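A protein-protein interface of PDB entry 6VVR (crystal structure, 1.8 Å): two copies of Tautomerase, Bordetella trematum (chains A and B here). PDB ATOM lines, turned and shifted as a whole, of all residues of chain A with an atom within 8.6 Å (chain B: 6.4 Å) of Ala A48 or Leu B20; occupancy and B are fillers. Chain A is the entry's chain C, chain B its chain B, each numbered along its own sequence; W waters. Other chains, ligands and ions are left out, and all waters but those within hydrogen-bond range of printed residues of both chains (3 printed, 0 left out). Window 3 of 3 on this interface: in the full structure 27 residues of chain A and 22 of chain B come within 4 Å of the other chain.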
ATOM      1  N   MET A   8      28.533 -21.259 -37.004  1.00  0.00           N
ATOM      2  CA  MET A   8      28.633 -21.712 -35.623  1.00  0.00           C
ATOM      3  C   MET A   8      29.365 -23.046 -35.545  1.00  0.00           C
ATOM      4  O   MET A   8      29.283 -23.881 -36.457  1.00  0.00           O
ATOM      5  CB  MET A   8      27.244 -21.850 -35.000  1.00  0.00           C
ATOM      6  CG  MET A   8      26.365 -20.604 -35.114  1.00  0.00           C
ATOM      7  SD  MET A   8      27.182 -19.109 -34.502  1.00  0.00           S
ATOM      8  CE  MET A   8      27.337 -19.499 -32.752  1.00  0.00           C
ATOM      9  N   GLN A   9      30.097 -23.237 -34.447  1.00  0.00           N
ATOM     10  CA  GLN A   9      30.668 -24.544 -34.156  1.00  0.00           C
ATOM     11  C   GLN A   9      29.555 -25.573 -34.022  1.00  0.00           C
ATOM     12  O   GLN A   9      28.407 -25.240 -33.723  1.00  0.00           O
ATOM     13  CB  GLN A   9      31.476 -24.509 -32.855  1.00  0.00           C
ATOM     14  CG  GLN A   9      32.822 -23.831 -32.941  1.00  0.00           C
ATOM     15  CD  GLN A   9      33.506 -23.744 -31.586  1.00  0.00           C
ATOM     16  OE1 GLN A   9      32.911 -24.064 -30.558  1.00  0.00           O
ATOM     17  NE2 GLN A   9      34.760 -23.310 -31.581  1.00  0.00           N
ATOM     18  N   TYR A  45      32.687 -20.463 -35.093  1.00  0.00           N
ATOM     19  CA  TYR A  45      32.577 -19.594 -33.923  1.00  0.00           C
ATOM     20  C   TYR A  45      31.833 -20.300 -32.799  1.00  0.00           C
ATOM     21  O   TYR A  45      30.790 -20.919 -33.033  1.00  0.00           O
ATOM     22  CB  TYR A  45      31.837 -18.293 -34.253  1.00  0.00           C
ATOM     23  CG  TYR A  45      32.584 -17.425 -35.219  1.00  0.00           C
ATOM     24  CD1 TYR A  45      32.625 -17.746 -36.569  1.00  0.00           C
ATOM     25  CD2 TYR A  45      33.245 -16.286 -34.789  1.00  0.00           C
ATOM     26  CE1 TYR A  45      33.321 -16.969 -37.461  1.00  0.00           C
ATOM     27  CE2 TYR A  45      33.939 -15.496 -35.681  1.00  0.00           C
ATOM     28  CZ  TYR A  45      33.967 -15.846 -37.020  1.00  0.00           C
ATOM     29  OH  TYR A  45      34.642 -15.064 -37.919  1.00  0.00           O
ATOM     30  N   ALA A  46      32.349 -20.174 -31.579  1.00  0.00           N
ATOM     31  CA  ALA A  46      31.585 -20.619 -30.424  1.00  0.00           C
ATOM     32  C   ALA A  46      30.421 -19.667 -30.177  1.00  0.00           C
ATOM     33  O   ALA A  46      30.476 -18.483 -30.519  1.00  0.00           O
ATOM     34  CB  ALA A  46      32.470 -20.699 -29.183  1.00  0.00           C
ATOM     35  N   ALA A  47      29.352 -20.199 -29.583  1.00  0.00           N
ATOM     36  CA  ALA A  47      28.198 -19.363 -29.265  1.00  0.00           C
ATOM     37  C   ALA A  47      28.602 -18.164 -28.420  1.00  0.00           C
ATOM     38  O   ALA A  47      28.071 -17.064 -28.596  1.00  0.00           O
ATOM     39  CB  ALA A  47      27.137 -20.189 -28.551  1.00  0.00           C
ATOM     40  N   ALA A  48      29.575 -18.346 -27.529  1.00  0.00           N
ATOM     41  CA  ALA A  48      30.004 -17.253 -26.667  1.00  0.00           C
ATOM     42  C   ALA A  48      30.628 -16.101 -27.449  1.00  0.00           C
ATOM     43  O   ALA A  48      30.712 -14.990 -26.918  1.00  0.00           O
ATOM     44  CB  ALA A  48      30.997 -17.760 -25.617  1.00  0.00           C
ATOM     45  N   ASP A  49      31.031 -16.335 -28.700  1.00  0.00           N
ATOM     46  CA  ASP A  49      31.729 -15.347 -29.511  1.00  0.00           C
ATOM     47  C   ASP A  49      30.805 -14.549 -30.428  1.00  0.00           C
ATOM     48  O   ASP A  49      31.300 -13.799 -31.272  1.00  0.00           O
ATOM     49  CB  ASP A  49      32.810 -16.005 -30.380  1.00  0.00           C
ATOM     50  CG  ASP A  49      33.766 -16.881 -29.597  1.00  0.00           C
ATOM     51  OD1 ASP A  49      34.060 -16.557 -28.440  1.00  0.00           O
ATOM     52  OD2 ASP A  49      34.256 -17.876 -30.176  1.00  0.00           O
ATOM     53  N   VAL A  50      29.487 -14.694 -30.310  1.00  0.00           N
ATOM     54  CA  VAL A  50      28.582 -13.993 -31.214  1.00  0.00           C
ATOM     55  C   VAL A  50      27.482 -13.283 -30.431  1.00  0.00           C
ATOM     56  O   VAL A  50      27.055 -13.726 -29.360  1.00  0.00           O
ATOM     57  CB  VAL A  50      27.967 -14.937 -32.281  1.00  0.00           C
ATOM     58  CG1 VAL A  50      29.047 -15.769 -32.963  1.00  0.00           C
ATOM     59  CG2 VAL A  50      26.948 -15.832 -31.670  1.00  0.00           C
ATOM     60  N   ILE A  51      27.024 -12.162 -30.987  1.00  0.00           N
ATOM     61  CA  ILE A  51      25.861 -11.438 -30.490  1.00  0.00           C
ATOM     62  C   ILE A  51      25.022 -11.043 -31.698  1.00  0.00           C
ATOM     63  O   ILE A  51      25.556 -10.575 -32.711  1.00  0.00           O
ATOM     64  CB  ILE A  51      26.262 -10.208 -29.638  1.00  0.00           C
ATOM     65  CG1 ILE A  51      25.037  -9.569 -28.971  1.00  0.00           C
ATOM     66  CG2 ILE A  51      27.043  -9.173 -30.471  1.00  0.00           C
ATOM     67  CD1 ILE A  51      25.399  -8.567 -27.878  1.00  0.00           C
ATOM     68  N   VAL A  52      23.714 -11.281 -31.621  1.00  0.00           N
ATOM     69  CA  VAL A  52      22.803 -10.946 -32.710  1.00  0.00           C
ATOM     70  C   VAL A  52      21.620 -10.207 -32.100  1.00  0.00           C
ATOM     71  O   VAL A  52      20.937 -10.753 -31.227  1.00  0.00           O
ATOM     72  CB  VAL A  52      22.326 -12.192 -33.483  1.00  0.00           C
ATOM     73  CG1 VAL A  52      21.283 -11.807 -34.527  1.00  0.00           C
ATOM     74  CG2 VAL A  52      23.500 -12.921 -34.160  1.00  0.00           C
ATOM     75  N   GLY A  54      21.453  -7.981 -29.929  1.00  0.00           N
ATOM     76  CA  GLY A  54      21.609  -7.854 -28.500  1.00  0.00           C
ATOM     77  C   GLY A  54      21.665  -9.158 -27.738  1.00  0.00           C
ATOM     78  O   GLY A  54      21.948  -9.134 -26.536  1.00  0.00           O
ATOM     79  N   GLU A  55      21.405 -10.292 -28.388  1.00  0.00           N
ATOM     80  CA  GLU A  55      21.381 -11.593 -27.726  1.00  0.00           C
ATOM     81  C   GLU A  55      22.729 -12.281 -27.906  1.00  0.00           C
ATOM     82  O   GLU A  55      23.083 -12.684 -29.016  1.00  0.00           O
ATOM     83  CB  GLU A  55      20.254 -12.459 -28.285  1.00  0.00           C
ATOM     84  CG  GLU A  55      18.863 -11.849 -28.123  1.00  0.00           C
ATOM     85  CD  GLU A  55      18.535 -11.514 -26.675  1.00  0.00           C
ATOM     86  OE1 GLU A  55      18.828 -12.344 -25.785  1.00  0.00           O
ATOM     87  OE2 GLU A  55      17.986 -10.419 -26.423  1.00  0.00           O
ATOM     88  N   VAL A  56      23.475 -12.434 -26.814  1.00  0.00           N
ATOM     89  CA  VAL A  56      24.746 -13.143 -26.882  1.00  0.00           C
ATOM     90  C   VAL A  56      24.469 -14.629 -27.065  1.00  0.00           C
ATOM     91  O   VAL A  56      23.624 -15.201 -26.370  1.00  0.00           O
ATOM     92  CB  VAL A  56      25.585 -12.885 -25.620  1.00  0.00           C
ATOM     93  CG1 VAL A  56      26.887 -13.679 -25.688  1.00  0.00           C
ATOM     94  CG2 VAL A  56      25.872 -11.403 -25.467  1.00  0.00           C
ATOM     95  N   GLY A  57      25.156 -15.250 -28.027  1.00  0.00           N
ATOM     96  CA  GLY A  57      25.022 -16.674 -28.266  1.00  0.00           C
ATOM     97  C   GLY A  57      24.011 -17.074 -29.320  1.00  0.00           C
ATOM     98  O   GLY A  57      23.854 -18.277 -29.573  1.00  0.00           O
ATOM     99  N   ALA A  58      23.314 -16.115 -29.931  1.00  0.00           N
ATOM    100  CA  ALA A  58      22.363 -16.423 -30.993  1.00  0.00           C
ATOM    101  C   ALA A  58      23.079 -16.993 -32.208  1.00  0.00           C
ATOM    102  O   ALA A  58      24.038 -16.399 -32.704  1.00  0.00           O
ATOM    103  CB  ALA A  58      21.596 -15.168 -31.398  1.00  0.00           C
ATOM    104  N   VAL B   5      35.016  -8.742 -35.138  1.00  0.00           N
ATOM    105  CA  VAL B   5      35.942  -8.170 -34.170  1.00  0.00           C
ATOM    106  C   VAL B   5      37.095  -9.137 -33.975  1.00  0.00           C
ATOM    107  O   VAL B   5      36.887 -10.353 -33.903  1.00  0.00           O
ATOM    108  CB  VAL B   5      35.241  -7.900 -32.832  1.00  0.00           C
ATOM    109  CG1 VAL B   5      36.148  -7.078 -31.932  1.00  0.00           C
ATOM    110  CG2 VAL B   5      33.903  -7.225 -33.085  1.00  0.00           C
ATOM    111  N   ALA B  15      34.890 -10.487 -19.853  1.00  0.00           N
ATOM    112  CA  ALA B  15      35.335  -9.350 -20.657  1.00  0.00           C
ATOM    113  C   ALA B  15      34.841  -9.469 -22.095  1.00  0.00           C
ATOM    114  O   ALA B  15      34.448  -8.472 -22.708  1.00  0.00           O
ATOM    115  CB  ALA B  15      36.866  -9.237 -20.638  1.00  0.00           C
ATOM    116  N   LYS B  16      34.861 -10.680 -22.652  1.00  0.00           N
ATOM    117  CA  LYS B  16      34.447 -10.843 -24.040  1.00  0.00           C
ATOM    118  C   LYS B  16      32.938 -10.662 -24.189  1.00  0.00           C
ATOM    119  O   LYS B  16      32.481 -10.079 -25.180  1.00  0.00           O
ATOM    120  CB  LYS B  16      34.906 -12.198 -24.564  1.00  0.00           C
ATOM    121  CG  LYS B  16      36.419 -12.290 -24.651  1.00  0.00           C
ATOM    122  CD  LYS B  16      36.870 -13.594 -25.282  1.00  0.00           C
ATOM    123  CE  LYS B  16      36.988 -14.694 -24.241  1.00  0.00           C
ATOM    124  NZ  LYS B  16      37.378 -15.983 -24.893  1.00  0.00           N
ATOM    125  N   THR B  17      32.149 -11.137 -23.211  1.00  0.00           N
ATOM    126  CA  THR B  17      30.711 -10.851 -23.219  1.00  0.00           C
ATOM    127  C   THR B  17      30.455  -9.355 -23.119  1.00  0.00           C
ATOM    128  O   THR B  17      29.620  -8.804 -23.851  1.00  0.00           O
ATOM    129  CB  THR B  17      29.995 -11.569 -22.070  1.00  0.00           C
ATOM    130  OG1 THR B  17      30.144 -12.987 -22.210  1.00  0.00           O
ATOM    131  CG2 THR B  17      28.497 -11.219 -22.087  1.00  0.00           C
ATOM    132  N   ALA B  18      31.158  -8.681 -22.202  1.00  0.00           N
ATOM    133  CA  ALA B  18      31.002  -7.234 -22.080  1.00  0.00           C
ATOM    134  C   ALA B  18      31.367  -6.540 -23.384  1.00  0.00           C
ATOM    135  O   ALA B  18      30.711  -5.573 -23.786  1.00  0.00           O
ATOM    136  CB  ALA B  18      31.854  -6.701 -20.931  1.00  0.00           C
ATOM    137  N   LEU B  19      32.403  -7.039 -24.067  1.00  0.00           N
ATOM    138  CA  LEU B  19      32.829  -6.451 -25.336  1.00  0.00           C
ATOM    139  C   LEU B  19      31.738  -6.568 -26.400  1.00  0.00           C
ATOM    140  O   LEU B  19      31.409  -5.588 -27.078  1.00  0.00           O
ATOM    141  CB  LEU B  19      34.117  -7.124 -25.810  1.00  0.00           C
ATOM    142  CG  LEU B  19      34.541  -6.804 -27.244  1.00  0.00           C
ATOM    143  CD1 LEU B  19      35.042  -5.364 -27.310  1.00  0.00           C
ATOM    144  CD2 LEU B  19      35.605  -7.774 -27.749  1.00  0.00           C
ATOM    145  N   LEU B  20      31.165  -7.763 -26.565  1.00  0.00           N
ATOM    146  CA  LEU B  20      30.100  -7.925 -27.555  1.00  0.00           C
ATOM    147  C   LEU B  20      28.916  -7.011 -27.254  1.00  0.00           C
ATOM    148  O   LEU B  20      28.373  -6.363 -28.159  1.00  0.00           O
ATOM    149  CB  LEU B  20      29.650  -9.385 -27.616  1.00  0.00           C
ATOM    150  CG  LEU B  20      30.697 -10.352 -28.175  1.00  0.00           C
ATOM    151  CD1 LEU B  20      30.304 -11.790 -27.870  1.00  0.00           C
ATOM    152  CD2 LEU B  20      30.869 -10.149 -29.680  1.00  0.00           C
ATOM    153  N   LYS B  21      28.505  -6.943 -25.986  1.00  0.00           N
ATOM    154  CA  LYS B  21      27.385  -6.091 -25.613  1.00  0.00           C
ATOM    155  C   LYS B  21      27.719  -4.617 -25.808  1.00  0.00           C
ATOM    156  O   LYS B  21      26.879  -3.844 -26.274  1.00  0.00           O
ATOM    157  CB  LYS B  21      26.994  -6.363 -24.162  1.00  0.00           C
ATOM    158  CG  LYS B  21      26.300  -7.697 -23.968  1.00  0.00           C
ATOM    159  CD  LYS B  21      26.023  -7.942 -22.488  1.00  0.00           C
ATOM    160  CE  LYS B  21      24.888  -8.932 -22.299  1.00  0.00           C
ATOM    161  NZ  LYS B  21      24.715  -9.274 -20.858  1.00  0.00           N
ATOM    162  N   ALA B  22      28.940  -4.211 -25.461  1.00  0.00           N
ATOM    163  CA  ALA B  22      29.320  -2.807 -25.592  1.00  0.00           C
ATOM    164  C   ALA B  22      29.415  -2.391 -27.051  1.00  0.00           C
ATOM    165  O   ALA B  22      29.074  -1.251 -27.401  1.00  0.00           O
ATOM    166  CB  ALA B  22      30.649  -2.552 -24.892  1.00  0.00           C
ATOM    167  N   LEU B  23      29.904  -3.287 -27.915  1.00  0.00           N
ATOM    168  CA  LEU B  23      29.965  -2.963 -29.335  1.00  0.00           C
ATOM    169  C   LEU B  23      28.566  -2.789 -29.901  1.00  0.00           C
ATOM    170  O   LEU B  23      28.294  -1.827 -30.637  1.00  0.00           O
ATOM    171  CB  LEU B  23      30.719  -4.047 -30.098  1.00  0.00           C
ATOM    172  CG  LEU B  23      32.227  -4.123 -29.824  1.00  0.00           C
ATOM    173  CD1 LEU B  23      32.773  -5.441 -30.318  1.00  0.00           C
ATOM    174  CD2 LEU B  23      32.964  -2.953 -30.476  1.00  0.00           C
ATOM    175  N   SER B  24      27.662  -3.716 -29.565  1.00  0.00           N
ATOM    176  CA  SER B  24      26.284  -3.613 -30.038  1.00  0.00           C
ATOM    177  C   SER B  24      25.651  -2.311 -29.562  1.00  0.00           C
ATOM    178  O   SER B  24      25.055  -1.569 -30.357  1.00  0.00           O
ATOM    179  CB  SER B  24      25.483  -4.836 -29.569  1.00  0.00           C
ATOM    180  OG  SER B  24      24.118  -4.759 -29.947  1.00  0.00           O
ATOM    181  N   ASP B  25      25.808  -2.000 -28.268  1.00  0.00           N
ATOM    182  CA  ASP B  25      25.267  -0.760 -27.709  1.00  0.00           C
ATOM    183  C   ASP B  25      25.851   0.453 -28.409  1.00  0.00           C
ATOM    184  O   ASP B  25      25.146   1.439 -28.658  1.00  0.00           O
ATOM    185  CB  ASP B  25      25.578  -0.655 -26.217  1.00  0.00           C
ATOM    186  CG  ASP B  25      24.676  -1.503 -25.358  1.00  0.00           C
ATOM    187  OD1 ASP B  25      23.641  -1.984 -25.863  1.00  0.00           O
ATOM    188  OD2 ASP B  25      25.012  -1.671 -24.159  1.00  0.00           O
ATOM    189  N   ALA B  40      27.545  -8.888 -34.157  1.00  0.00           N
ATOM    190  CA  ALA B  40      28.995  -8.878 -34.020  1.00  0.00           C
ATOM    191  C   ALA B  40      29.470 -10.291 -33.736  1.00  0.00           C
ATOM    192  O   ALA B  40      28.821 -11.036 -33.000  1.00  0.00           O
ATOM    193  CB  ALA B  40      29.471  -7.942 -32.903  1.00  0.00           C
ATOM    194  N   ILE B  41      30.597 -10.662 -34.334  1.00  0.00           N
ATOM    195  CA  ILE B  41      31.220 -11.956 -34.096  1.00  0.00           C
ATOM    196  C   ILE B  41      32.688 -11.703 -33.801  1.00  0.00           C
ATOM    197  O   ILE B  41      33.296 -10.762 -34.325  1.00  0.00           O
ATOM    198  CB  ILE B  41      31.042 -12.936 -35.282  1.00  0.00           C
ATOM    199  CG1 ILE B  41      31.785 -12.446 -36.533  1.00  0.00           C
ATOM    200  CG2 ILE B  41      29.559 -13.166 -35.576  1.00  0.00           C
ATOM    201  CD1 ILE B  41      31.544 -13.334 -37.755  1.00  0.00           C
ATOM    202  N   LEU B  42      33.258 -12.554 -32.957  1.00  0.00           N
ATOM    203  CA  LEU B  42      34.552 -12.315 -32.340  1.00  0.00           C
ATOM    204  C   LEU B  42      35.533 -13.430 -32.675  1.00  0.00           C
ATOM    205  O   LEU B  42      35.175 -14.611 -32.637  1.00  0.00           O
ATOM    206  CB  LEU B  42      34.371 -12.220 -30.821  1.00  0.00           C
ATOM    207  CG  LEU B  42      35.526 -12.122 -29.851  1.00  0.00           C
ATOM    208  CD1 LEU B  42      36.458 -11.033 -30.316  1.00  0.00           C
ATOM    209  CD2 LEU B  42      34.929 -11.769 -28.502  1.00  0.00           C
ATOM    210  N   SER B  90      36.028  -2.337 -22.441  1.00  0.00           N
ATOM    211  CA  SER B  90      35.666  -3.723 -22.155  1.00  0.00           C
ATOM    212  C   SER B  90      36.894  -4.586 -21.906  1.00  0.00           C
ATOM    213  O   SER B  90      36.866  -5.478 -21.052  1.00  0.00           O
ATOM    214  CB  SER B  90      34.846  -4.296 -23.309  1.00  0.00           C
ATOM    215  OG  SER B  90      33.685  -3.513 -23.520  1.00  0.00           O
HETATM  216  O   HOH W   1      29.938 -14.528 -24.305  1.00  0.00           O
HETATM  217  O   HOH W   2      23.797  -7.163 -31.413  1.00  0.00           O
HETATM  218  O   HOH W   3      36.116 -17.219 -32.822  1.00  0.00           O
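Ala A48 touches just one residue of chain B: Leu B20. Of chain A, only Ala A48 (3.4 Å), Asp A49 (3.8 Å), Val A50 (3.9 Å) and Ile A51 (3.7 Å) come within 4 Å of Leu B20. Printed residues of chain A within 4 Å of Ile B41: Tyr A45, Asp A49 and Val A50. Printed residues of chain B within 4 Å of Ile A51: Leu B20, Lys B21 and Ala B40. Of the printed residues of chain B, Asp A49 touches Leu B20 (3.8 Å), Ile B41 (3.4 Å) and Leu B42 (2.9 Å). Ala A58 touches none of the printed residues of chain B. Val A56 touches none of the printed residues of chain B. The nearest residue of chain B that does not touch Ala A48 is Thr B17 (5.1 Å).
No position is printed for both chains. Of the 12 pairs that touch across the chains among the printed residues, none has its exchanged pair printed and touching as well.
Of the 15 printed residues of chain A, 5 touch a printed residue of chain B.
Water W1 bridges OG1 of Thr B17 (2.6 Å) and O of Ala A48 (2.8 Å). Water W3 bridges the backbone carbonyl oxygen (O) of Leu B42 (2.8 Å) and the side-chain carboxylate (OD2) of Asp A49 (3.3 Å). Water W2 lies within hydrogen-bond range of OG of Ser B24 (2.8 Å) and N of Gly A54 (2.9 Å).
O of Ala B40 sits at hydrogen-bond distance from N of Ile A51, 2.9 Å away. The backbone NH of Leu B42 sits at hydrogen-bond distance from the backbone carbonyl oxygen of Asp A49.
N of Val B5 is in hydrogen-bond range of O of Ile B41, at 2.8 Å. O of Tyr A45 is in hydrogen-bond range of N of Gln A9 (2.8 Å). The backbone NH (N) of Ala A46 is in hydrogen-bond range of the side-chain carboxylate (OD2) of Asp A49, at 3.3 Å. The backbone carbonyl oxygen (O) of Val A50 is in hydrogen-bond range of the backbone NH (N) of Gly A57 (2.8 Å).
Among the printed residues, merely in contact across the chains: Tyr A45 with Ile B41 (3.6 Å), Tyr A45 with Leu B42 (3.3 Å), Ala A48 with Leu B20 (3.4 Å), Asp A49 with Leu B20 (3.8 Å), Asp A49 with Ile B41 (3.4 Å), Val A50 with Leu B20 (3.9 Å), Val A50 with Ala B40 (3.5 Å), Val A50 with Ile B41 (3.7 Å), Ile A51 with Leu B20 (3.7 Å) and Ile A51 with Lys B21 (3.9 Å).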
